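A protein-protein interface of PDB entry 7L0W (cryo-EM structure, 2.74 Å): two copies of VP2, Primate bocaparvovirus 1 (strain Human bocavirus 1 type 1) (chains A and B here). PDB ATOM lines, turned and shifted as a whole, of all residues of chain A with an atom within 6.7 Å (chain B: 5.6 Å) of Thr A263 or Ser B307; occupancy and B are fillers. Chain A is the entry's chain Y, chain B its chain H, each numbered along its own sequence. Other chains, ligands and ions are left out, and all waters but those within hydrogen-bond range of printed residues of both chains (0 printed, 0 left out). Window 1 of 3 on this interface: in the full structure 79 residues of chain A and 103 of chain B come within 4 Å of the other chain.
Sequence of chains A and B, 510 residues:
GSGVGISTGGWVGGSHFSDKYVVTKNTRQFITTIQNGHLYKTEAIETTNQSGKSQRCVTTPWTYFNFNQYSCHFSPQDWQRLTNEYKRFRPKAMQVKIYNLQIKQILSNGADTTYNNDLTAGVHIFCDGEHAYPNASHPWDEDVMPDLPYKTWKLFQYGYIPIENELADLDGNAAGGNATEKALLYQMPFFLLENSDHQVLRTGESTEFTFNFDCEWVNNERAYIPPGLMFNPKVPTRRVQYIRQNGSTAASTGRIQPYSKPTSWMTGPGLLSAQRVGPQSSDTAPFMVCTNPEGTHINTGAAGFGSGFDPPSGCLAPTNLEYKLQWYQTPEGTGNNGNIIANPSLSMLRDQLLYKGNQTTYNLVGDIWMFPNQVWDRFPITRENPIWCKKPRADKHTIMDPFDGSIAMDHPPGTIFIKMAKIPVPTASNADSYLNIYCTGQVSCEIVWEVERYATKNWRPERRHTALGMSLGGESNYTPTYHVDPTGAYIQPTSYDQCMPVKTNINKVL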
ATOM      1  N   PRO A 226       9.513  32.755 -11.076  1.00  0.00           N
ATOM      2  CA  PRO A 226       9.234  32.483  -9.680  1.00  0.00           C
ATOM      3  C   PRO A 226      10.505  32.557  -8.862  1.00  0.00           C
ATOM      4  O   PRO A 226      11.603  32.354  -9.394  1.00  0.00           O
ATOM      5  CB  PRO A 226       8.681  31.055  -9.708  1.00  0.00           C
ATOM      6  CG  PRO A 226       8.157  30.894 -11.065  1.00  0.00           C
ATOM      7  CD  PRO A 226       9.094  31.641 -11.935  1.00  0.00           C
ATOM      8  N   PRO A 227      10.403  32.838  -7.566  1.00  0.00           N
ATOM      9  CA  PRO A 227      11.601  32.798  -6.721  1.00  0.00           C
ATOM     10  C   PRO A 227      12.258  31.434  -6.674  1.00  0.00           C
ATOM     11  O   PRO A 227      13.390  31.317  -6.196  1.00  0.00           O
ATOM     12  CB  PRO A 227      11.071  33.233  -5.352  1.00  0.00           C
ATOM     13  CG  PRO A 227       9.634  32.897  -5.388  1.00  0.00           C
ATOM     14  CD  PRO A 227       9.199  33.162  -6.791  1.00  0.00           C
ATOM     15  N   GLY A 228      11.581  30.390  -7.141  1.00  0.00           N
ATOM     16  CA  GLY A 228      12.190  29.073  -7.150  1.00  0.00           C
ATOM     17  C   GLY A 228      13.240  28.896  -8.226  1.00  0.00           C
ATOM     18  O   GLY A 228      14.142  28.070  -8.085  1.00  0.00           O
ATOM     19  N   LEU A 229      13.174  29.701  -9.279  1.00  0.00           N
ATOM     20  CA  LEU A 229      14.148  29.598 -10.362  1.00  0.00           C
ATOM     21  C   LEU A 229      15.322  30.552 -10.204  1.00  0.00           C
ATOM     22  O   LEU A 229      16.095  30.744 -11.127  1.00  0.00           O
ATOM     23  CB  LEU A 229      13.479  29.830 -11.708  1.00  0.00           C
ATOM     24  CG  LEU A 229      12.305  28.915 -12.023  1.00  0.00           C
ATOM     25  CD1 LEU A 229      11.847  29.161 -13.446  1.00  0.00           C
ATOM     26  CD2 LEU A 229      12.717  27.471 -11.833  1.00  0.00           C
ATOM     27  N   MET A 230      15.461  31.138  -9.027  1.00  0.00           N
ATOM     28  CA  MET A 230      16.541  32.074  -8.763  1.00  0.00           C
ATOM     29  C   MET A 230      17.929  31.454  -8.792  1.00  0.00           C
ATOM     30  O   MET A 230      18.894  32.090  -8.388  1.00  0.00           O
ATOM     31  CB  MET A 230      16.348  32.720  -7.405  1.00  0.00           C
ATOM     32  CG  MET A 230      15.313  33.818  -7.355  1.00  0.00           C
ATOM     33  SD  MET A 230      15.466  34.663  -5.778  1.00  0.00           S
ATOM     34  CE  MET A 230      16.841  35.755  -6.104  1.00  0.00           C
ATOM     35  N   PHE A 231      18.042  30.215  -9.248  1.00  0.00           N
ATOM     36  CA  PHE A 231      19.349  29.577  -9.294  1.00  0.00           C
ATOM     37  C   PHE A 231      19.952  29.617 -10.697  1.00  0.00           C
ATOM     38  O   PHE A 231      19.426  30.239 -11.622  1.00  0.00           O
ATOM     39  CB  PHE A 231      19.241  28.134  -8.821  1.00  0.00           C
ATOM     40  CG  PHE A 231      18.306  27.310  -9.638  1.00  0.00           C
ATOM     41  CD1 PHE A 231      18.755  26.616 -10.734  1.00  0.00           C
ATOM     42  CD2 PHE A 231      16.976  27.242  -9.313  1.00  0.00           C
ATOM     43  CE1 PHE A 231      17.899  25.871 -11.481  1.00  0.00           C
ATOM     44  CE2 PHE A 231      16.116  26.496 -10.062  1.00  0.00           C
ATOM     45  CZ  PHE A 231      16.578  25.814 -11.146  1.00  0.00           C
ATOM     46  N   SER A 260      17.183  21.343 -11.671  1.00  0.00           N
ATOM     47  CA  SER A 260      16.184  21.583 -10.633  1.00  0.00           C
ATOM     48  C   SER A 260      16.891  21.612  -9.290  1.00  0.00           C
ATOM     49  O   SER A 260      17.203  20.570  -8.720  1.00  0.00           O
ATOM     50  CB  SER A 260      15.126  20.518 -10.676  1.00  0.00           C
ATOM     51  OG  SER A 260      15.703  19.257 -10.413  1.00  0.00           O
ATOM     52  N   LYS A 261      17.114  22.806  -8.768  1.00  0.00           N
ATOM     53  CA  LYS A 261      17.659  22.954  -7.437  1.00  0.00           C
ATOM     54  C   LYS A 261      16.551  23.178  -6.421  1.00  0.00           C
ATOM     55  O   LYS A 261      15.470  23.659  -6.764  1.00  0.00           O
ATOM     56  CB  LYS A 261      18.662  24.095  -7.409  1.00  0.00           C
ATOM     57  CG  LYS A 261      19.908  23.782  -8.199  1.00  0.00           C
ATOM     58  CD  LYS A 261      20.871  24.930  -8.176  1.00  0.00           C
ATOM     59  CE  LYS A 261      22.113  24.603  -8.950  1.00  0.00           C
ATOM     60  NZ  LYS A 261      23.042  25.755  -8.956  1.00  0.00           N
ATOM     61  N   PRO A 262      16.794  22.836  -5.158  1.00  0.00           N
ATOM     62  CA  PRO A 262      15.793  23.105  -4.126  1.00  0.00           C
ATOM     63  C   PRO A 262      15.609  24.596  -3.940  1.00  0.00           C
ATOM     64  O   PRO A 262      16.561  25.375  -4.005  1.00  0.00           O
ATOM     65  CB  PRO A 262      16.399  22.466  -2.877  1.00  0.00           C
ATOM     66  CG  PRO A 262      17.340  21.479  -3.387  1.00  0.00           C
ATOM     67  CD  PRO A 262      17.927  22.076  -4.614  1.00  0.00           C
ATOM     68  N   THR A 263      14.368  24.997  -3.707  1.00  0.00           N
ATOM     69  CA  THR A 263      14.051  26.381  -3.403  1.00  0.00           C
ATOM     70  C   THR A 263      13.955  26.544  -1.896  1.00  0.00           C
ATOM     71  O   THR A 263      13.493  25.641  -1.194  1.00  0.00           O
ATOM     72  CB  THR A 263      12.756  26.829  -4.084  1.00  0.00           C
ATOM     73  OG1 THR A 263      12.550  28.222  -3.839  1.00  0.00           O
ATOM     74  CG2 THR A 263      11.573  26.067  -3.569  1.00  0.00           C
ATOM     75  N   SER A 264      14.429  27.671  -1.402  1.00  0.00           N
ATOM     76  CA  SER A 264      14.283  28.009  -0.001  1.00  0.00           C
ATOM     77  C   SER A 264      13.002  28.770   0.270  1.00  0.00           C
ATOM     78  O   SER A 264      12.766  29.173   1.409  1.00  0.00           O
ATOM     79  CB  SER A 264      15.483  28.834   0.464  1.00  0.00           C
ATOM     80  OG  SER A 264      15.342  29.219   1.814  1.00  0.00           O
ATOM     81  N   TRP A 265      12.175  28.965  -0.748  1.00  0.00           N
ATOM     82  CA  TRP A 265      11.037  29.861  -0.696  1.00  0.00           C
ATOM     83  C   TRP A 265       9.763  29.076  -0.961  1.00  0.00           C
ATOM     84  O   TRP A 265       9.760  28.089  -1.693  1.00  0.00           O
ATOM     85  CB  TRP A 265      11.217  30.985  -1.713  1.00  0.00           C
ATOM     86  CG  TRP A 265      12.514  31.645  -1.494  1.00  0.00           C
ATOM     87  CD1 TRP A 265      13.627  31.543  -2.266  1.00  0.00           C
ATOM     88  CD2 TRP A 265      12.890  32.396  -0.348  1.00  0.00           C
ATOM     89  NE1 TRP A 265      14.658  32.250  -1.701  1.00  0.00           N
ATOM     90  CE2 TRP A 265      14.227  32.775  -0.515  1.00  0.00           C
ATOM     91  CE3 TRP A 265      12.213  32.813   0.793  1.00  0.00           C
ATOM     92  CZ2 TRP A 265      14.899  33.548   0.415  1.00  0.00           C
ATOM     93  CZ3 TRP A 265      12.875  33.574   1.712  1.00  0.00           C
ATOM     94  CH2 TRP A 265      14.203  33.940   1.521  1.00  0.00           C
ATOM     95  N   MET A 266       8.669  29.530  -0.366  1.00  0.00           N
ATOM     96  CA  MET A 266       7.434  28.771  -0.396  1.00  0.00           C
ATOM     97  C   MET A 266       6.285  29.669  -0.826  1.00  0.00           C
ATOM     98  O   MET A 266       6.420  30.889  -0.934  1.00  0.00           O
ATOM     99  CB  MET A 266       7.158  28.120   0.963  1.00  0.00           C
ATOM    100  CG  MET A 266       5.963  27.195   1.007  1.00  0.00           C
ATOM    101  SD  MET A 266       5.986  26.160   2.457  1.00  0.00           S
ATOM    102  CE  MET A 266       4.391  25.400   2.345  1.00  0.00           C
ATOM    103  N   HIS B 138      23.840  30.717  -5.922  1.00  0.00           N
ATOM    104  CA  HIS B 138      22.727  30.061  -5.272  1.00  0.00           C
ATOM    105  C   HIS B 138      23.321  29.136  -4.225  1.00  0.00           C
ATOM    106  O   HIS B 138      24.411  28.593  -4.432  1.00  0.00           O
ATOM    107  CB  HIS B 138      21.869  29.271  -6.268  1.00  0.00           C
ATOM    108  CG  HIS B 138      20.635  28.680  -5.669  1.00  0.00           C
ATOM    109  ND1 HIS B 138      20.625  27.450  -5.055  1.00  0.00           N
ATOM    110  CD2 HIS B 138      19.375  29.161  -5.572  1.00  0.00           C
ATOM    111  CE1 HIS B 138      19.405  27.189  -4.620  1.00  0.00           C
ATOM    112  NE2 HIS B 138      18.629  28.212  -4.921  1.00  0.00           N
ATOM    113  N   ASP B 283      12.677  16.487 -10.601  1.00  0.00           N
ATOM    114  CA  ASP B 283      12.745  17.163  -9.314  1.00  0.00           C
ATOM    115  C   ASP B 283      11.901  16.403  -8.302  1.00  0.00           C
ATOM    116  O   ASP B 283      10.693  16.229  -8.485  1.00  0.00           O
ATOM    117  CB  ASP B 283      12.253  18.598  -9.449  1.00  0.00           C
ATOM    118  CG  ASP B 283      12.441  19.401  -8.185  1.00  0.00           C
ATOM    119  OD1 ASP B 283      13.597  19.723  -7.846  1.00  0.00           O
ATOM    120  OD2 ASP B 283      11.438  19.710  -7.518  1.00  0.00           O
ATOM    121  N   PHE B 287       7.494  18.881  -1.484  1.00  0.00           N
ATOM    122  CA  PHE B 287       6.583  19.949  -1.868  1.00  0.00           C
ATOM    123  C   PHE B 287       7.116  20.654  -3.100  1.00  0.00           C
ATOM    124  O   PHE B 287       8.325  20.847  -3.236  1.00  0.00           O
ATOM    125  CB  PHE B 287       6.398  20.966  -0.745  1.00  0.00           C
ATOM    126  CG  PHE B 287       5.687  20.427   0.448  1.00  0.00           C
ATOM    127  CD1 PHE B 287       4.311  20.391   0.486  1.00  0.00           C
ATOM    128  CD2 PHE B 287       6.390  19.959   1.534  1.00  0.00           C
ATOM    129  CE1 PHE B 287       3.655  19.894   1.580  1.00  0.00           C
ATOM    130  CE2 PHE B 287       5.734  19.463   2.630  1.00  0.00           C
ATOM    131  CZ  PHE B 287       4.366  19.429   2.651  1.00  0.00           C
ATOM    132  N   MET B 288       6.209  21.046  -3.989  1.00  0.00           N
ATOM    133  CA  MET B 288       6.549  21.794  -5.190  1.00  0.00           C
ATOM    134  C   MET B 288       5.940  23.179  -5.112  1.00  0.00           C
ATOM    135  O   MET B 288       4.719  23.317  -5.032  1.00  0.00           O
ATOM    136  CB  MET B 288       6.041  21.105  -6.446  1.00  0.00           C
ATOM    137  CG  MET B 288       6.632  19.764  -6.682  1.00  0.00           C
ATOM    138  SD  MET B 288       8.413  19.815  -6.769  1.00  0.00           S
ATOM    139  CE  MET B 288       8.594  20.853  -8.195  1.00  0.00           C
ATOM    140  N   VAL B 289       6.785  24.196  -5.158  1.00  0.00           N
ATOM    141  CA  VAL B 289       6.344  25.579  -5.228  1.00  0.00           C
ATOM    142  C   VAL B 289       6.282  25.954  -6.697  1.00  0.00           C
ATOM    143  O   VAL B 289       7.315  26.010  -7.373  1.00  0.00           O
ATOM    144  CB  VAL B 289       7.285  26.510  -4.454  1.00  0.00           C
ATOM    145  CG1 VAL B 289       6.834  27.945  -4.601  1.00  0.00           C
ATOM    146  CG2 VAL B 289       7.331  26.107  -3.002  1.00  0.00           C
ATOM    147  N   CYS B 290       5.077  26.208  -7.193  1.00  0.00           N
ATOM    148  CA  CYS B 290       4.873  26.406  -8.616  1.00  0.00           C
ATOM    149  C   CYS B 290       3.939  27.577  -8.860  1.00  0.00           C
ATOM    150  O   CYS B 290       3.250  28.054  -7.957  1.00  0.00           O
ATOM    151  CB  CYS B 290       4.314  25.144  -9.273  1.00  0.00           C
ATOM    152  SG  CYS B 290       2.883  24.472  -8.466  1.00  0.00           S
ATOM    153  N   PHE B 305       6.303  21.710 -13.712  1.00  0.00           N
ATOM    154  CA  PHE B 305       6.282  23.134 -13.436  1.00  0.00           C
ATOM    155  C   PHE B 305       6.412  23.330 -11.935  1.00  0.00           C
ATOM    156  O   PHE B 305       5.737  22.658 -11.151  1.00  0.00           O
ATOM    157  CB  PHE B 305       5.000  23.785 -13.968  1.00  0.00           C
ATOM    158  CG  PHE B 305       3.749  23.327 -13.280  1.00  0.00           C
ATOM    159  CD1 PHE B 305       3.167  24.098 -12.295  1.00  0.00           C
ATOM    160  CD2 PHE B 305       3.174  22.115 -13.589  1.00  0.00           C
ATOM    161  CE1 PHE B 305       2.017  23.680 -11.658  1.00  0.00           C
ATOM    162  CE2 PHE B 305       2.027  21.692 -12.951  1.00  0.00           C
ATOM    163  CZ  PHE B 305       1.450  22.476 -11.984  1.00  0.00           C
ATOM    164  N   GLY B 306       7.303  24.223 -11.539  1.00  0.00           N
ATOM    165  CA  GLY B 306       7.546  24.446 -10.133  1.00  0.00           C
ATOM    166  C   GLY B 306       8.877  23.876  -9.679  1.00  0.00           C
ATOM    167  O   GLY B 306       9.463  22.991 -10.304  1.00  0.00           O
ATOM    168  N   SER B 307       9.359  24.408  -8.564  1.00  0.00           N
ATOM    169  CA  SER B 307      10.629  24.009  -7.982  1.00  0.00           C
ATOM    170  C   SER B 307      10.376  23.448  -6.596  1.00  0.00           C
ATOM    171  O   SER B 307       9.524  23.955  -5.863  1.00  0.00           O
ATOM    172  CB  SER B 307      11.591  25.188  -7.904  1.00  0.00           C
ATOM    173  OG  SER B 307      11.089  26.169  -7.025  1.00  0.00           O
ATOM    174  N   GLY B 308      11.121  22.409  -6.239  1.00  0.00           N
ATOM    175  CA  GLY B 308      10.820  21.697  -5.016  1.00  0.00           C
ATOM    176  C   GLY B 308      11.326  22.436  -3.793  1.00  0.00           C
ATOM    177  O   GLY B 308      12.400  23.038  -3.804  1.00  0.00           O
ATOM    178  N   PHE B 309      10.547  22.366  -2.724  1.00  0.00           N
ATOM    179  CA  PHE B 309      10.854  23.024  -1.462  1.00  0.00           C
ATOM    180  C   PHE B 309      11.365  21.955  -0.499  1.00  0.00           C
ATOM    181  O   PHE B 309      10.604  21.128  -0.003  1.00  0.00           O
ATOM    182  CB  PHE B 309       9.623  23.733  -0.931  1.00  0.00           C
ATOM    183  CG  PHE B 309       9.815  24.369   0.403  1.00  0.00           C
ATOM    184  CD1 PHE B 309      10.439  25.589   0.516  1.00  0.00           C
ATOM    185  CD2 PHE B 309       9.354  23.754   1.543  1.00  0.00           C
ATOM    186  CE1 PHE B 309      10.609  26.173   1.742  1.00  0.00           C
ATOM    187  CE2 PHE B 309       9.524  24.336   2.765  1.00  0.00           C
ATOM    188  CZ  PHE B 309      10.152  25.546   2.866  1.00  0.00           C
ATOM    189  N   ASP B 310      12.666  21.988  -0.234  1.00  0.00           N
ATOM    190  CA  ASP B 310      13.307  21.013   0.634  1.00  0.00           C
ATOM    191  C   ASP B 310      14.449  21.678   1.386  1.00  0.00           C
ATOM    192  O   ASP B 310      15.114  22.542   0.831  1.00  0.00           O
ATOM    193  CB  ASP B 310      13.822  19.838  -0.192  1.00  0.00           C
ATOM    194  CG  ASP B 310      14.488  18.775   0.651  1.00  0.00           C
ATOM    195  OD1 ASP B 310      13.785  18.077   1.411  1.00  0.00           O
ATOM    196  OD2 ASP B 310      15.724  18.636   0.561  1.00  0.00           O
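Of the 12 printed residues of chain B, 7 touch a printed residue of chain A.
Printed residues of chain B that touch a printed residue of chain A: His B138, Asp B283, Val B289, Ser B307, Gly B308, Phe B309 and Asp B310.
Hydrophobic or aromatic side chains of chain B within 4 Å of the printed part of chain A: His B138, Val B289 and Phe B309.
Hydrophobic or aromatic side chains of chain A within 4 Å of the printed part of chain B: Phe A231, Pro A262 and Met A266.
Among the printed residues, no Asp or Glu carboxylate lies within 4 Å of a Lys or Arg side-chain nitrogen of the other chain.
Among the printed residues, merely in contact across the chains: Gly A228 with Ser B307, Trp A265 with Val B289, Trp A265 with Phe B309, Pro A262 with Gly B308, Phe A231 with His B138, Pro A262 with His B138, Thr A263 with Ser B307, Thr A263 with Phe B309, Ser A264 with Phe B309, Met A266 with Val B289, Thr A263 with Asp B310, Pro A262 with Asp B310 and Met A266 with Phe B309.
No position is printed for both chains.
Of the 15 pairs that touch across the chains among the printed residues, none has its exchanged pair printed and touching as well.
Of the printed residues of chain B, Pro A262 touches His B138 (3.4 Å), Gly B308 (3.4 Å) and Asp B310 (3.9 Å).
Thr A263 touches four residues of chain B.
Printed residues of chain B within 4 Å of Trp A265: Val B289 and Phe B309.
Of the printed residues of chain A, His B138 touches Phe A231 and Pro A262.
Ser B307 touches just these residues of chain A: Gly A228 (3.1 Å) and Thr A263 (3.4 Å).
The nearest residue of chain B that does not touch Thr A263 is Val B289 (4.3 Å).
The nearest residue of chain A that does not touch Ser B307 is Lys A261 (4.3 Å).
The side-chain carboxylate (OD1) of Asp B283 sits close to the side-chain hydroxyl (OG) of Ser A260, at 3.4 Å.
N of Thr A263 sits at hydrogen-bond distance from O of Gly B308 (2.8 Å).
The backbone NH (N) of Gly B308 sits at hydrogen-bond distance from the side-chain carboxylate (OD2) of Asp B283 (3.0 Å).
N of Phe B309 lies within hydrogen-bond range of O of Phe B287.
The backbone NH (N) of Gly B308 lies close to the side-chain sulfur (SD) of Met B288.
N of Val B289 is in hydrogen-bond range of O of Ser B307.
OG1 of Thr A263 lies within hydrogen-bond range of N of Trp A265, at 3.2 Å.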
